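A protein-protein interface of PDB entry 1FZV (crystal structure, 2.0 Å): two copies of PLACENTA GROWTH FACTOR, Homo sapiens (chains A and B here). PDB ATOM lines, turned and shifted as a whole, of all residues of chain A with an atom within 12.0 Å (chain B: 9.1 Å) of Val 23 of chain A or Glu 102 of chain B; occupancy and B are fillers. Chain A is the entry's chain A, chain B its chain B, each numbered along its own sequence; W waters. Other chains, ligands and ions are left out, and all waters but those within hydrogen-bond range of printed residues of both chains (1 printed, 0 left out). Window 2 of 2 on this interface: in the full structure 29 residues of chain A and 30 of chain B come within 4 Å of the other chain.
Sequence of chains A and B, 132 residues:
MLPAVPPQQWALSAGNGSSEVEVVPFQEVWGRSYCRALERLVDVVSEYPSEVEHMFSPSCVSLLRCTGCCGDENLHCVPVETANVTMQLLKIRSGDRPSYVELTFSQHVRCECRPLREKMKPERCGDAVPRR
Of chain B, only Thr 86 (3.5 Å), Gln 88 (3.9 Å) and Glu 102 (3.5 Å) come within 4 Å of Val 23 of chain A. Of chain A, only Val 23 (3.5 Å) comes within 4 Å of Glu 102 of chain B. Of chain B, only Thr 86 (2.9 Å), Met 87 (3.8 Å) and Gln 88 (2.9 Å) come within 4 Å of Val 24 of chain A. Thr 86 of chain B touches just these residues of chain A: Val 21, Glu 22, Val 23 and Val 24. Of chain A, only Val 23, Val 24, Pro 25, Phe 26 and Val 29 come within 4 Å of Gln 88 of chain B. No residue of chain A comes within 4 Å of Val 101 of chain B. Leu 103 of chain B touches none of the printed residues of chain A. Thr 104 of chain B touches none of the printed residues of chain A. Printed residues of chain B within 4 Å of Val 29 of chain A: Met 87 (3.9 Å), Gln 88 (3.8 Å) and Leu 89 (3.9 Å). Printed residues of chain B within 4 Å of Pro 25 of chain A: Gln 88 (3.8 Å). Printed residues of chain B within 4 Å of Phe 26 of chain A: Gln 88 (3.1 Å), Leu 90 (3.8 Å) and Tyr 100 (3.5 Å). Printed residues of chain A within 4 Å of Tyr 100 of chain B: Phe 26. The nearest residue of chain B that does not touch Val 23 of chain A is Met 87 of chain B (4.4 Å). The nearest residue of chain A that does not touch Glu 102 of chain B is Val 24 of chain A (6.9 Å).
Val 21 of chain A touches Thr 86 of chain B. O of Thr 86 of chain B touches O of Glu 22 of chain A, at 3.6 Å. Thr 86 of chain B touches Val 23 of chain A (O to CA, 3.5 Å). Val 23 of chain A touches Glu 102 of chain B. Val 24 of chain A touches Met 87 of chain B. Pro 25 of chain A touches Gln 88 of chain B (CA to OE1, 3.8 Å). CE1 of Phe 26 of chain A touches CB of Leu 90 of chain B, at 3.8 Å. CG of Phe 26 of chain A touches CE2 of Tyr 100 of chain B (3.5 Å). CG2 of Val 29 of chain A touches CB of Met 87 of chain B, 3.9 Å away. Val 29 of chain A touches Leu 89 of chain B (CG1 to CD1, 3.9 Å).
The backbone carbonyl oxygen (O) of Thr 86 of chain B sits at hydrogen-bond distance from the backbone NH (N) of Val 24 of chain A. O of Val 24 of chain A is in hydrogen-bond range of N of Gln 88 of chain B. The backbone NH of Phe 26 of chain A lies within hydrogen-bond range of the side-chain amide oxygen of Gln 88 of chain B, 3.1 Å away.
The side-chain hydroxyl of Thr 104 of chain B lies within hydrogen-bond range of the side-chain hydroxyl of Thr 86 of chain B (2.7 Å). N of Met 87 of chain B sits at hydrogen-bond distance from O of Leu 103 of chain B, at 2.6 Å. O of Leu 89 of chain B sits at hydrogen-bond distance from N of Val 101 of chain B (2.6 Å).
No position is printed for both chains. Of the 15 pairs that touch across the chains among the printed residues, none has its exchanged pair printed and touching as well.
Of the 14 printed residues of chain A, 7 touch a printed residue of chain B. Printed residues of chain A that touch a printed residue of chain B: Val 21, Glu 22, Val 23, Val 24, Pro 25, Phe 26 and Val 29. Along chain A the printed residues that touch a printed residue of chain B span positions 21 to 29. Of the 17 printed residues of chain B, 7 touch a printed residue of chain A. Printed residues of chain B that touch a printed residue of chain A: Thr 86, Met 87, Gln 88, Leu 89, Leu 90, Tyr 100 and Glu 102. Hydrophobic or aromatic side chains of chain B within 4 Å of the printed part of chain A: Met 87, Leu 89, Leu 90 and Tyr 100.
Water W1 bridges O of Glu 22 of chain A (2.7 Å) and N of Thr 86 of chain B (2.9 Å).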
ATOM      1  N   SER A  18       3.334 -33.007   0.750  1.00  0.00           N
ATOM      2  CA  SER A  18       3.593 -32.047   1.864  1.00  0.00           C
ATOM      3  C   SER A  18       4.046 -30.708   1.300  1.00  0.00           C
ATOM      4  O   SER A  18       3.657 -29.646   1.799  1.00  0.00           O
ATOM      5  CB  SER A  18       4.663 -32.609   2.811  1.00  0.00           C
ATOM      6  N   SER A  19       4.866 -30.763   0.254  1.00  0.00           N
ATOM      7  CA  SER A  19       5.375 -29.557  -0.391  1.00  0.00           C
ATOM      8  C   SER A  19       4.389 -29.076  -1.468  1.00  0.00           C
ATOM      9  O   SER A  19       4.707 -28.182  -2.260  1.00  0.00           O
ATOM     10  CB  SER A  19       6.751 -29.842  -1.020  1.00  0.00           C
ATOM     11  OG  SER A  19       7.401 -28.645  -1.434  1.00  0.00           O
ATOM     12  N   GLU A  20       3.196 -29.671  -1.492  1.00  0.00           N
ATOM     13  CA  GLU A  20       2.169 -29.296  -2.469  1.00  0.00           C
ATOM     14  C   GLU A  20       1.162 -28.305  -1.889  1.00  0.00           C
ATOM     15  O   GLU A  20       0.450 -28.593  -0.935  1.00  0.00           O
ATOM     16  CB  GLU A  20       1.462 -30.543  -2.997  1.00  0.00           C
ATOM     17  CG  GLU A  20       0.999 -31.509  -1.934  1.00  0.00           C
ATOM     18  CD  GLU A  20       1.259 -32.950  -2.339  1.00  0.00           C
ATOM     19  OE1 GLU A  20       0.984 -33.291  -3.515  1.00  0.00           O
ATOM     20  OE2 GLU A  20       1.732 -33.741  -1.488  1.00  0.00           O
ATOM     21  N   VAL A  21       1.119 -27.125  -2.484  1.00  0.00           N
ATOM     22  CA  VAL A  21       0.251 -26.060  -2.026  1.00  0.00           C
ATOM     23  C   VAL A  21      -1.097 -26.030  -2.729  1.00  0.00           C
ATOM     24  O   VAL A  21      -1.247 -26.541  -3.834  1.00  0.00           O
ATOM     25  CB  VAL A  21       0.939 -24.697  -2.230  1.00  0.00           C
ATOM     26  CG1 VAL A  21       1.258 -24.493  -3.691  1.00  0.00           C
ATOM     27  CG2 VAL A  21       0.053 -23.582  -1.739  1.00  0.00           C
ATOM     28  N   GLU A  22      -2.073 -25.433  -2.059  1.00  0.00           N
ATOM     29  CA  GLU A  22      -3.403 -25.282  -2.605  1.00  0.00           C
ATOM     30  C   GLU A  22      -3.390 -24.223  -3.715  1.00  0.00           C
ATOM     31  O   GLU A  22      -2.640 -23.235  -3.651  1.00  0.00           O
ATOM     32  CB  GLU A  22      -4.363 -24.850  -1.511  1.00  0.00           C
ATOM     33  CG  GLU A  22      -5.665 -24.262  -2.033  1.00  0.00           C
ATOM     34  CD  GLU A  22      -6.568 -23.790  -0.923  1.00  0.00           C
ATOM     35  OE1 GLU A  22      -7.621 -23.198  -1.223  1.00  0.00           O
ATOM     36  OE2 GLU A  22      -6.219 -24.014   0.259  1.00  0.00           O
ATOM     37  N   VAL A  23      -4.210 -24.445  -4.742  1.00  0.00           N
ATOM     38  CA  VAL A  23      -4.319 -23.501  -5.839  1.00  0.00           C
ATOM     39  C   VAL A  23      -5.720 -22.918  -5.799  1.00  0.00           C
ATOM     40  O   VAL A  23      -6.704 -23.657  -5.821  1.00  0.00           O
ATOM     41  CB  VAL A  23      -4.119 -24.183  -7.211  1.00  0.00           C
ATOM     42  CG1 VAL A  23      -4.332 -23.147  -8.349  1.00  0.00           C
ATOM     43  CG2 VAL A  23      -2.738 -24.813  -7.281  1.00  0.00           C
ATOM     44  N   VAL A  24      -5.830 -21.601  -5.716  1.00  0.00           N
ATOM     45  CA  VAL A  24      -7.153 -21.007  -5.707  1.00  0.00           C
ATOM     46  C   VAL A  24      -7.645 -21.049  -7.187  1.00  0.00           C
ATOM     47  O   VAL A  24      -7.024 -20.464  -8.071  1.00  0.00           O
ATOM     48  CB  VAL A  24      -7.111 -19.563  -5.201  1.00  0.00           C
ATOM     49  CG1 VAL A  24      -8.520 -18.962  -5.272  1.00  0.00           C
ATOM     50  CG2 VAL A  24      -6.563 -19.530  -3.722  1.00  0.00           C
ATOM     51  N   PRO A  25      -8.756 -21.752  -7.453  1.00  0.00           N
ATOM     52  CA  PRO A  25      -9.333 -21.890  -8.809  1.00  0.00           C
ATOM     53  C   PRO A  25      -9.715 -20.555  -9.432  1.00  0.00           C
ATOM     54  O   PRO A  25     -10.158 -19.644  -8.743  1.00  0.00           O
ATOM     55  CB  PRO A  25     -10.566 -22.775  -8.581  1.00  0.00           C
ATOM     56  CG  PRO A  25     -10.313 -23.430  -7.231  1.00  0.00           C
ATOM     57  CD  PRO A  25      -9.668 -22.329  -6.450  1.00  0.00           C
ATOM     58  N   PHE A  26      -9.547 -20.451 -10.742  1.00  0.00           N
ATOM     59  CA  PHE A  26      -9.886 -19.249 -11.499  1.00  0.00           C
ATOM     60  C   PHE A  26     -11.206 -18.585 -11.103  1.00  0.00           C
ATOM     61  O   PHE A  26     -11.261 -17.374 -10.928  1.00  0.00           O
ATOM     62  CB  PHE A  26      -9.932 -19.587 -13.009  1.00  0.00           C
ATOM     63  CG  PHE A  26     -10.326 -18.421 -13.892  1.00  0.00           C
ATOM     64  CD1 PHE A  26      -9.477 -17.327 -14.058  1.00  0.00           C
ATOM     65  CD2 PHE A  26     -11.549 -18.428 -14.575  1.00  0.00           C
ATOM     66  CE1 PHE A  26      -9.834 -16.248 -14.900  1.00  0.00           C
ATOM     67  CE2 PHE A  26     -11.917 -17.362 -15.413  1.00  0.00           C
ATOM     68  CZ  PHE A  26     -11.067 -16.273 -15.581  1.00  0.00           C
ATOM     69  N   GLN A  27     -12.274 -19.369 -10.998  1.00  0.00           N
ATOM     70  CA  GLN A  27     -13.581 -18.808 -10.650  1.00  0.00           C
ATOM     71  C   GLN A  27     -13.530 -18.065  -9.317  1.00  0.00           C
ATOM     72  O   GLN A  27     -14.095 -16.979  -9.182  1.00  0.00           O
ATOM     73  CB  GLN A  27     -14.643 -19.911 -10.551  1.00  0.00           C
ATOM     74  CG  GLN A  27     -14.913 -20.655 -11.856  1.00  0.00           C
ATOM     75  CD  GLN A  27     -15.978 -20.004 -12.715  1.00  0.00           C
ATOM     76  OE1 GLN A  27     -16.499 -20.627 -13.638  1.00  0.00           O
ATOM     77  NE2 GLN A  27     -16.305 -18.750 -12.423  1.00  0.00           N
ATOM     78  N   GLU A  28     -12.863 -18.662  -8.335  1.00  0.00           N
ATOM     79  CA  GLU A  28     -12.749 -18.034  -7.020  1.00  0.00           C
ATOM     80  C   GLU A  28     -11.908 -16.772  -7.124  1.00  0.00           C
ATOM     81  O   GLU A  28     -12.290 -15.710  -6.627  1.00  0.00           O
ATOM     82  CB  GLU A  28     -12.136 -19.002  -6.002  1.00  0.00           C
ATOM     83  CG  GLU A  28     -12.684 -18.750  -4.605  1.00  0.00           C
ATOM     84  CD  GLU A  28     -11.929 -19.462  -3.495  1.00  0.00           C
ATOM     85  OE1 GLU A  28     -11.528 -20.628  -3.698  1.00  0.00           O
ATOM     86  OE2 GLU A  28     -11.766 -18.848  -2.407  1.00  0.00           O
ATOM     87  N   VAL A  29     -10.777 -16.873  -7.807  1.00  0.00           N
ATOM     88  CA  VAL A  29      -9.900 -15.729  -7.967  1.00  0.00           C
ATOM     89  C   VAL A  29     -10.710 -14.564  -8.525  1.00  0.00           C
ATOM     90  O   VAL A  29     -10.767 -13.471  -7.934  1.00  0.00           O
ATOM     91  CB  VAL A  29      -8.724 -16.063  -8.918  1.00  0.00           C
ATOM     92  CG1 VAL A  29      -7.863 -14.845  -9.138  1.00  0.00           C
ATOM     93  CG2 VAL A  29      -7.916 -17.207  -8.363  1.00  0.00           C
ATOM     94  N   TRP A  30     -11.354 -14.805  -9.669  1.00  0.00           N
ATOM     95  CA  TRP A  30     -12.156 -13.783 -10.333  1.00  0.00           C
ATOM     96  C   TRP A  30     -13.249 -13.216  -9.445  1.00  0.00           C
ATOM     97  O   TRP A  30     -13.437 -12.012  -9.388  1.00  0.00           O
ATOM     98  CB  TRP A  30     -12.786 -14.359 -11.619  1.00  0.00           C
ATOM     99  CG  TRP A  30     -13.665 -13.384 -12.343  1.00  0.00           C
ATOM    100  CD1 TRP A  30     -14.930 -12.982 -11.976  1.00  0.00           C
ATOM    101  CD2 TRP A  30     -13.360 -12.687 -13.549  1.00  0.00           C
ATOM    102  NE1 TRP A  30     -15.422 -12.082 -12.884  1.00  0.00           N
ATOM    103  CE2 TRP A  30     -14.483 -11.883 -13.865  1.00  0.00           C
ATOM    104  CE3 TRP A  30     -12.251 -12.662 -14.398  1.00  0.00           C
ATOM    105  CZ2 TRP A  30     -14.529 -11.058 -15.012  1.00  0.00           C
ATOM    106  CZ3 TRP A  30     -12.296 -11.839 -15.544  1.00  0.00           C
ATOM    107  CH2 TRP A  30     -13.429 -11.052 -15.835  1.00  0.00           C
ATOM    108  N   ARG A  32     -13.421 -13.206  -6.156  1.00  0.00           N
ATOM    109  CA  ARG A  32     -12.855 -12.515  -4.999  1.00  0.00           C
ATOM    110  C   ARG A  32     -12.419 -11.084  -5.322  1.00  0.00           C
ATOM    111  O   ARG A  32     -12.575 -10.176  -4.505  1.00  0.00           O
ATOM    112  CB  ARG A  32     -11.652 -13.298  -4.476  1.00  0.00           C
ATOM    113  CG  ARG A  32     -11.198 -12.841  -3.116  1.00  0.00           C
ATOM    114  CD  ARG A  32     -12.036 -13.497  -2.056  1.00  0.00           C
ATOM    115  NE  ARG A  32     -11.845 -12.894  -0.742  1.00  0.00           N
ATOM    116  CZ  ARG A  32     -12.324 -13.421   0.374  1.00  0.00           C
ATOM    117  NH1 ARG A  32     -13.006 -14.555   0.311  1.00  0.00           N
ATOM    118  NH2 ARG A  32     -12.131 -12.817   1.544  1.00  0.00           N
ATOM    119  N   TYR B  48       4.775  -7.759 -10.216  1.00  0.00           N
ATOM    120  CA  TYR B  48       5.962  -8.263 -10.886  1.00  0.00           C
ATOM    121  C   TYR B  48       7.072  -7.248 -10.711  1.00  0.00           C
ATOM    122  O   TYR B  48       6.828  -6.040 -10.726  1.00  0.00           O
ATOM    123  CB  TYR B  48       5.736  -8.489 -12.391  1.00  0.00           C
ATOM    124  CG  TYR B  48       5.215  -9.864 -12.737  1.00  0.00           C
ATOM    125  CD1 TYR B  48       3.876 -10.190 -12.551  1.00  0.00           C
ATOM    126  CD2 TYR B  48       6.069 -10.846 -13.241  1.00  0.00           C
ATOM    127  CE1 TYR B  48       3.397 -11.466 -12.864  1.00  0.00           C
ATOM    128  CE2 TYR B  48       5.598 -12.126 -13.558  1.00  0.00           C
ATOM    129  CZ  TYR B  48       4.263 -12.420 -13.367  1.00  0.00           C
ATOM    130  OH  TYR B  48       3.794 -13.661 -13.711  1.00  0.00           O
ATOM    131  N   PHE B  56      -3.078 -10.671 -17.922  1.00  0.00           N
ATOM    132  CA  PHE B  56      -3.757 -11.505 -16.934  1.00  0.00           C
ATOM    133  C   PHE B  56      -5.217 -11.193 -16.725  1.00  0.00           C
ATOM    134  O   PHE B  56      -5.629 -10.051 -16.804  1.00  0.00           O
ATOM    135  CB  PHE B  56      -3.032 -11.405 -15.576  1.00  0.00           C
ATOM    136  CG  PHE B  56      -1.582 -11.761 -15.650  1.00  0.00           C
ATOM    137  CD1 PHE B  56      -1.191 -13.087 -15.741  1.00  0.00           C
ATOM    138  CD2 PHE B  56      -0.616 -10.764 -15.718  1.00  0.00           C
ATOM    139  CE1 PHE B  56       0.148 -13.423 -15.904  1.00  0.00           C
ATOM    140  CE2 PHE B  56       0.720 -11.082 -15.881  1.00  0.00           C
ATOM    141  CZ  PHE B  56       1.105 -12.420 -15.977  1.00  0.00           C
ATOM    142  N   ASN B  84       2.531 -17.297   1.367  1.00  0.00           N
ATOM    143  CA  ASN B  84       2.266 -17.419  -0.071  1.00  0.00           C
ATOM    144  C   ASN B  84       0.850 -17.859  -0.358  1.00  0.00           C
ATOM    145  O   ASN B  84       0.225 -18.533   0.459  1.00  0.00           O
ATOM    146  CB  ASN B  84       3.175 -18.479  -0.688  1.00  0.00           C
ATOM    147  CG  ASN B  84       4.608 -18.066  -0.716  1.00  0.00           C
ATOM    148  OD1 ASN B  84       5.054 -17.431  -1.657  1.00  0.00           O
ATOM    149  ND2 ASN B  84       5.350 -18.407   0.345  1.00  0.00           N
ATOM    150  N   VAL B  85       0.365 -17.486  -1.542  1.00  0.00           N
ATOM    151  CA  VAL B  85      -0.939 -17.934  -2.008  1.00  0.00           C
ATOM    152  C   VAL B  85      -0.760 -18.167  -3.519  1.00  0.00           C
ATOM    153  O   VAL B  85      -0.229 -17.311  -4.226  1.00  0.00           O
ATOM    154  CB  VAL B  85      -2.058 -16.922  -1.740  1.00  0.00           C
ATOM    155  CG1 VAL B  85      -1.738 -15.581  -2.398  1.00  0.00           C
ATOM    156  CG2 VAL B  85      -3.391 -17.513  -2.242  1.00  0.00           C
ATOM    157  N   THR B  86      -1.132 -19.357  -3.992  1.00  0.00           N
ATOM    158  CA  THR B  86      -0.984 -19.682  -5.401  1.00  0.00           C
ATOM    159  C   THR B  86      -2.368 -19.583  -6.014  1.00  0.00           C
ATOM    160  O   THR B  86      -3.316 -20.195  -5.515  1.00  0.00           O
ATOM    161  CB  THR B  86      -0.427 -21.088  -5.582  1.00  0.00           C
ATOM    162  OG1 THR B  86       0.924 -21.117  -5.100  1.00  0.00           O
ATOM    163  CG2 THR B  86      -0.416 -21.481  -7.069  1.00  0.00           C
ATOM    164  N   MET B  87      -2.471 -18.787  -7.074  1.00  0.00           N
ATOM    165  CA  MET B  87      -3.751 -18.542  -7.732  1.00  0.00           C
ATOM    166  C   MET B  87      -3.756 -18.917  -9.213  1.00  0.00           C
ATOM    167  O   MET B  87      -2.759 -18.770  -9.904  1.00  0.00           O
ATOM    168  CB  MET B  87      -4.105 -17.070  -7.609  1.00  0.00           C
ATOM    169  CG  MET B  87      -4.529 -16.661  -6.217  1.00  0.00           C
ATOM    170  SD  MET B  87      -4.945 -14.948  -6.250  1.00  0.00           S
ATOM    171  CE  MET B  87      -4.421 -14.475  -4.503  1.00  0.00           C
ATOM    172  N   GLN B  88      -4.903 -19.376  -9.699  1.00  0.00           N
ATOM    173  CA  GLN B  88      -5.006 -19.759 -11.106  1.00  0.00           C
ATOM    174  C   GLN B  88      -5.592 -18.623 -11.930  1.00  0.00           C
ATOM    175  O   GLN B  88      -6.752 -18.271 -11.768  1.00  0.00           O
ATOM    176  CB  GLN B  88      -5.886 -21.001 -11.269  1.00  0.00           C
ATOM    177  CG  GLN B  88      -6.025 -21.393 -12.776  1.00  0.00           C
ATOM    178  CD  GLN B  88      -6.915 -22.586 -12.989  1.00  0.00           C
ATOM    179  OE1 GLN B  88      -8.022 -22.622 -12.273  1.00  0.00           O
ATOM    180  NE2 GLN B  88      -6.606 -23.480 -13.802  1.00  0.00           N
ATOM    181  N   LEU B  89      -4.785 -18.036 -12.801  1.00  0.00           N
ATOM    182  CA  LEU B  89      -5.272 -16.952 -13.617  1.00  0.00           C
ATOM    183  C   LEU B  89      -5.238 -17.355 -15.086  1.00  0.00           C
ATOM    184  O   LEU B  89      -4.630 -18.367 -15.472  1.00  0.00           O
ATOM    185  CB  LEU B  89      -4.432 -15.680 -13.433  1.00  0.00           C
ATOM    186  CG  LEU B  89      -4.805 -14.860 -12.176  1.00  0.00           C
ATOM    187  CD1 LEU B  89      -4.451 -15.668 -10.945  1.00  0.00           C
ATOM    188  CD2 LEU B  89      -4.096 -13.527 -12.164  1.00  0.00           C
ATOM    189  N   LEU B  90      -5.886 -16.520 -15.885  1.00  0.00           N
ATOM    190  CA  LEU B  90      -5.957 -16.728 -17.322  1.00  0.00           C
ATOM    191  C   LEU B  90      -4.944 -15.795 -17.959  1.00  0.00           C
ATOM    192  O   LEU B  90      -4.990 -14.583 -17.753  1.00  0.00           O
ATOM    193  CB  LEU B  90      -7.378 -16.419 -17.823  1.00  0.00           C
ATOM    194  CG  LEU B  90      -7.720 -16.605 -19.311  1.00  0.00           C
ATOM    195  CD1 LEU B  90      -7.506 -18.039 -19.751  1.00  0.00           C
ATOM    196  CD2 LEU B  90      -9.165 -16.235 -19.518  1.00  0.00           C
ATOM    197  N   LYS B  91      -4.000 -16.364 -18.697  1.00  0.00           N
ATOM    198  CA  LYS B  91      -3.005 -15.556 -19.381  1.00  0.00           C
ATOM    199  C   LYS B  91      -3.504 -15.310 -20.807  1.00  0.00           C
ATOM    200  O   LYS B  91      -3.838 -16.252 -21.531  1.00  0.00           O
ATOM    201  CB  LYS B  91      -1.662 -16.283 -19.414  1.00  0.00           C
ATOM    202  CG  LYS B  91      -0.575 -15.537 -20.152  1.00  0.00           C
ATOM    203  CD  LYS B  91       0.805 -16.010 -19.720  1.00  0.00           C
ATOM    204  CE  LYS B  91       0.986 -17.509 -19.920  1.00  0.00           C
ATOM    205  NZ  LYS B  91       1.036 -17.912 -21.361  1.00  0.00           N
ATOM    206  N   SER B  99      -4.654 -19.071 -22.014  1.00  0.00           N
ATOM    207  CA  SER B  99      -4.167 -20.222 -21.275  1.00  0.00           C
ATOM    208  C   SER B  99      -4.154 -19.953 -19.753  1.00  0.00           C
ATOM    209  O   SER B  99      -3.785 -18.877 -19.327  1.00  0.00           O
ATOM    210  CB  SER B  99      -2.756 -20.522 -21.760  1.00  0.00           C
ATOM    211  OG  SER B  99      -2.430 -21.869 -21.549  1.00  0.00           O
ATOM    212  N   TYR B 100      -4.565 -20.930 -18.950  1.00  0.00           N
ATOM    213  CA  TYR B 100      -4.576 -20.745 -17.499  1.00  0.00           C
ATOM    214  C   TYR B 100      -3.192 -20.983 -16.929  1.00  0.00           C
ATOM    215  O   TYR B 100      -2.485 -21.887 -17.377  1.00  0.00           O
ATOM    216  CB  TYR B 100      -5.568 -21.693 -16.835  1.00  0.00           C
ATOM    217  CG  TYR B 100      -6.998 -21.328 -17.136  1.00  0.00           C
ATOM    218  CD1 TYR B 100      -7.678 -21.885 -18.235  1.00  0.00           C
ATOM    219  CD2 TYR B 100      -7.645 -20.358 -16.376  1.00  0.00           C
ATOM    220  CE1 TYR B 100      -8.982 -21.467 -18.570  1.00  0.00           C
ATOM    221  CE2 TYR B 100      -8.920 -19.933 -16.694  1.00  0.00           C
ATOM    222  CZ  TYR B 100      -9.587 -20.488 -17.799  1.00  0.00           C
ATOM    223  OH  TYR B 100     -10.823 -20.000 -18.102  1.00  0.00           O
ATOM    224  N   VAL B 101      -2.806 -20.154 -15.958  1.00  0.00           N
ATOM    225  CA  VAL B 101      -1.506 -20.315 -15.316  1.00  0.00           C
ATOM    226  C   VAL B 101      -1.631 -20.208 -13.805  1.00  0.00           C
ATOM    227  O   VAL B 101      -2.563 -19.598 -13.279  1.00  0.00           O
ATOM    228  CB  VAL B 101      -0.466 -19.255 -15.774  1.00  0.00           C
ATOM    229  CG1 VAL B 101      -0.024 -19.531 -17.167  1.00  0.00           C
ATOM    230  CG2 VAL B 101      -1.029 -17.864 -15.621  1.00  0.00           C
ATOM    231  N   GLU B 102      -0.698 -20.831 -13.108  1.00  0.00           N
ATOM    232  CA  GLU B 102      -0.703 -20.774 -11.655  1.00  0.00           C
ATOM    233  C   GLU B 102       0.342 -19.747 -11.221  1.00  0.00           C
ATOM    234  O   GLU B 102       1.520 -19.859 -11.570  1.00  0.00           O
ATOM    235  CB  GLU B 102      -0.392 -22.152 -11.088  1.00  0.00           C
ATOM    236  CG  GLU B 102      -1.510 -23.154 -11.328  1.00  0.00           C
ATOM    237  CD  GLU B 102      -1.147 -24.542 -10.864  1.00  0.00           C
ATOM    238  OE1 GLU B 102       0.062 -24.813 -10.657  1.00  0.00           O
ATOM    239  OE2 GLU B 102      -2.055 -25.369 -10.699  1.00  0.00           O
ATOM    240  N   LEU B 103      -0.106 -18.719 -10.509  1.00  0.00           N
ATOM    241  CA  LEU B 103       0.791 -17.675 -10.046  1.00  0.00           C
ATOM    242  C   LEU B 103       0.814 -17.638  -8.526  1.00  0.00           C
ATOM    243  O   LEU B 103      -0.234 -17.676  -7.878  1.00  0.00           O
ATOM    244  CB  LEU B 103       0.368 -16.293 -10.574  1.00  0.00           C
ATOM    245  CG  LEU B 103       0.479 -15.925 -12.058  1.00  0.00           C
ATOM    246  CD1 LEU B 103       0.072 -14.487 -12.235  1.00  0.00           C
ATOM    247  CD2 LEU B 103       1.889 -16.111 -12.556  1.00  0.00           C
ATOM    248  N   THR B 104       2.020 -17.595  -7.969  1.00  0.00           N
ATOM    249  CA  THR B 104       2.198 -17.520  -6.521  1.00  0.00           C
ATOM    250  C   THR B 104       2.480 -16.077  -6.137  1.00  0.00           C
ATOM    251  O   THR B 104       3.377 -15.433  -6.683  1.00  0.00           O
ATOM    252  CB  THR B 104       3.347 -18.413  -6.046  1.00  0.00           C
ATOM    253  OG1 THR B 104       2.966 -19.783  -6.221  1.00  0.00           O
ATOM    254  CG2 THR B 104       3.667 -18.141  -4.530  1.00  0.00           C
ATOM    255  N   PHE B 105       1.688 -15.572  -5.205  1.00  0.00           N
ATOM    256  CA  PHE B 105       1.823 -14.214  -4.737  1.00  0.00           C
ATOM    257  C   PHE B 105       2.237 -14.175  -3.262  1.00  0.00           C
ATOM    258  O   PHE B 105       1.956 -15.090  -2.504  1.00  0.00           O
ATOM    259  CB  PHE B 105       0.495 -13.474  -4.840  1.00  0.00           C
ATOM    260  CG  PHE B 105      -0.023 -13.333  -6.259  1.00  0.00           C
ATOM    261  CD1 PHE B 105       0.305 -12.222  -7.023  1.00  0.00           C
ATOM    262  CD2 PHE B 105      -0.841 -14.315  -6.806  1.00  0.00           C
ATOM    263  CE1 PHE B 105      -0.193 -12.079  -8.342  1.00  0.00           C
ATOM    264  CE2 PHE B 105      -1.354 -14.195  -8.128  1.00  0.00           C
ATOM    265  CZ  PHE B 105      -1.027 -13.079  -8.889  1.00  0.00           C
HETATM  266  O   HOH W   1      -2.079 -21.219  -1.980  1.00  0.00           O
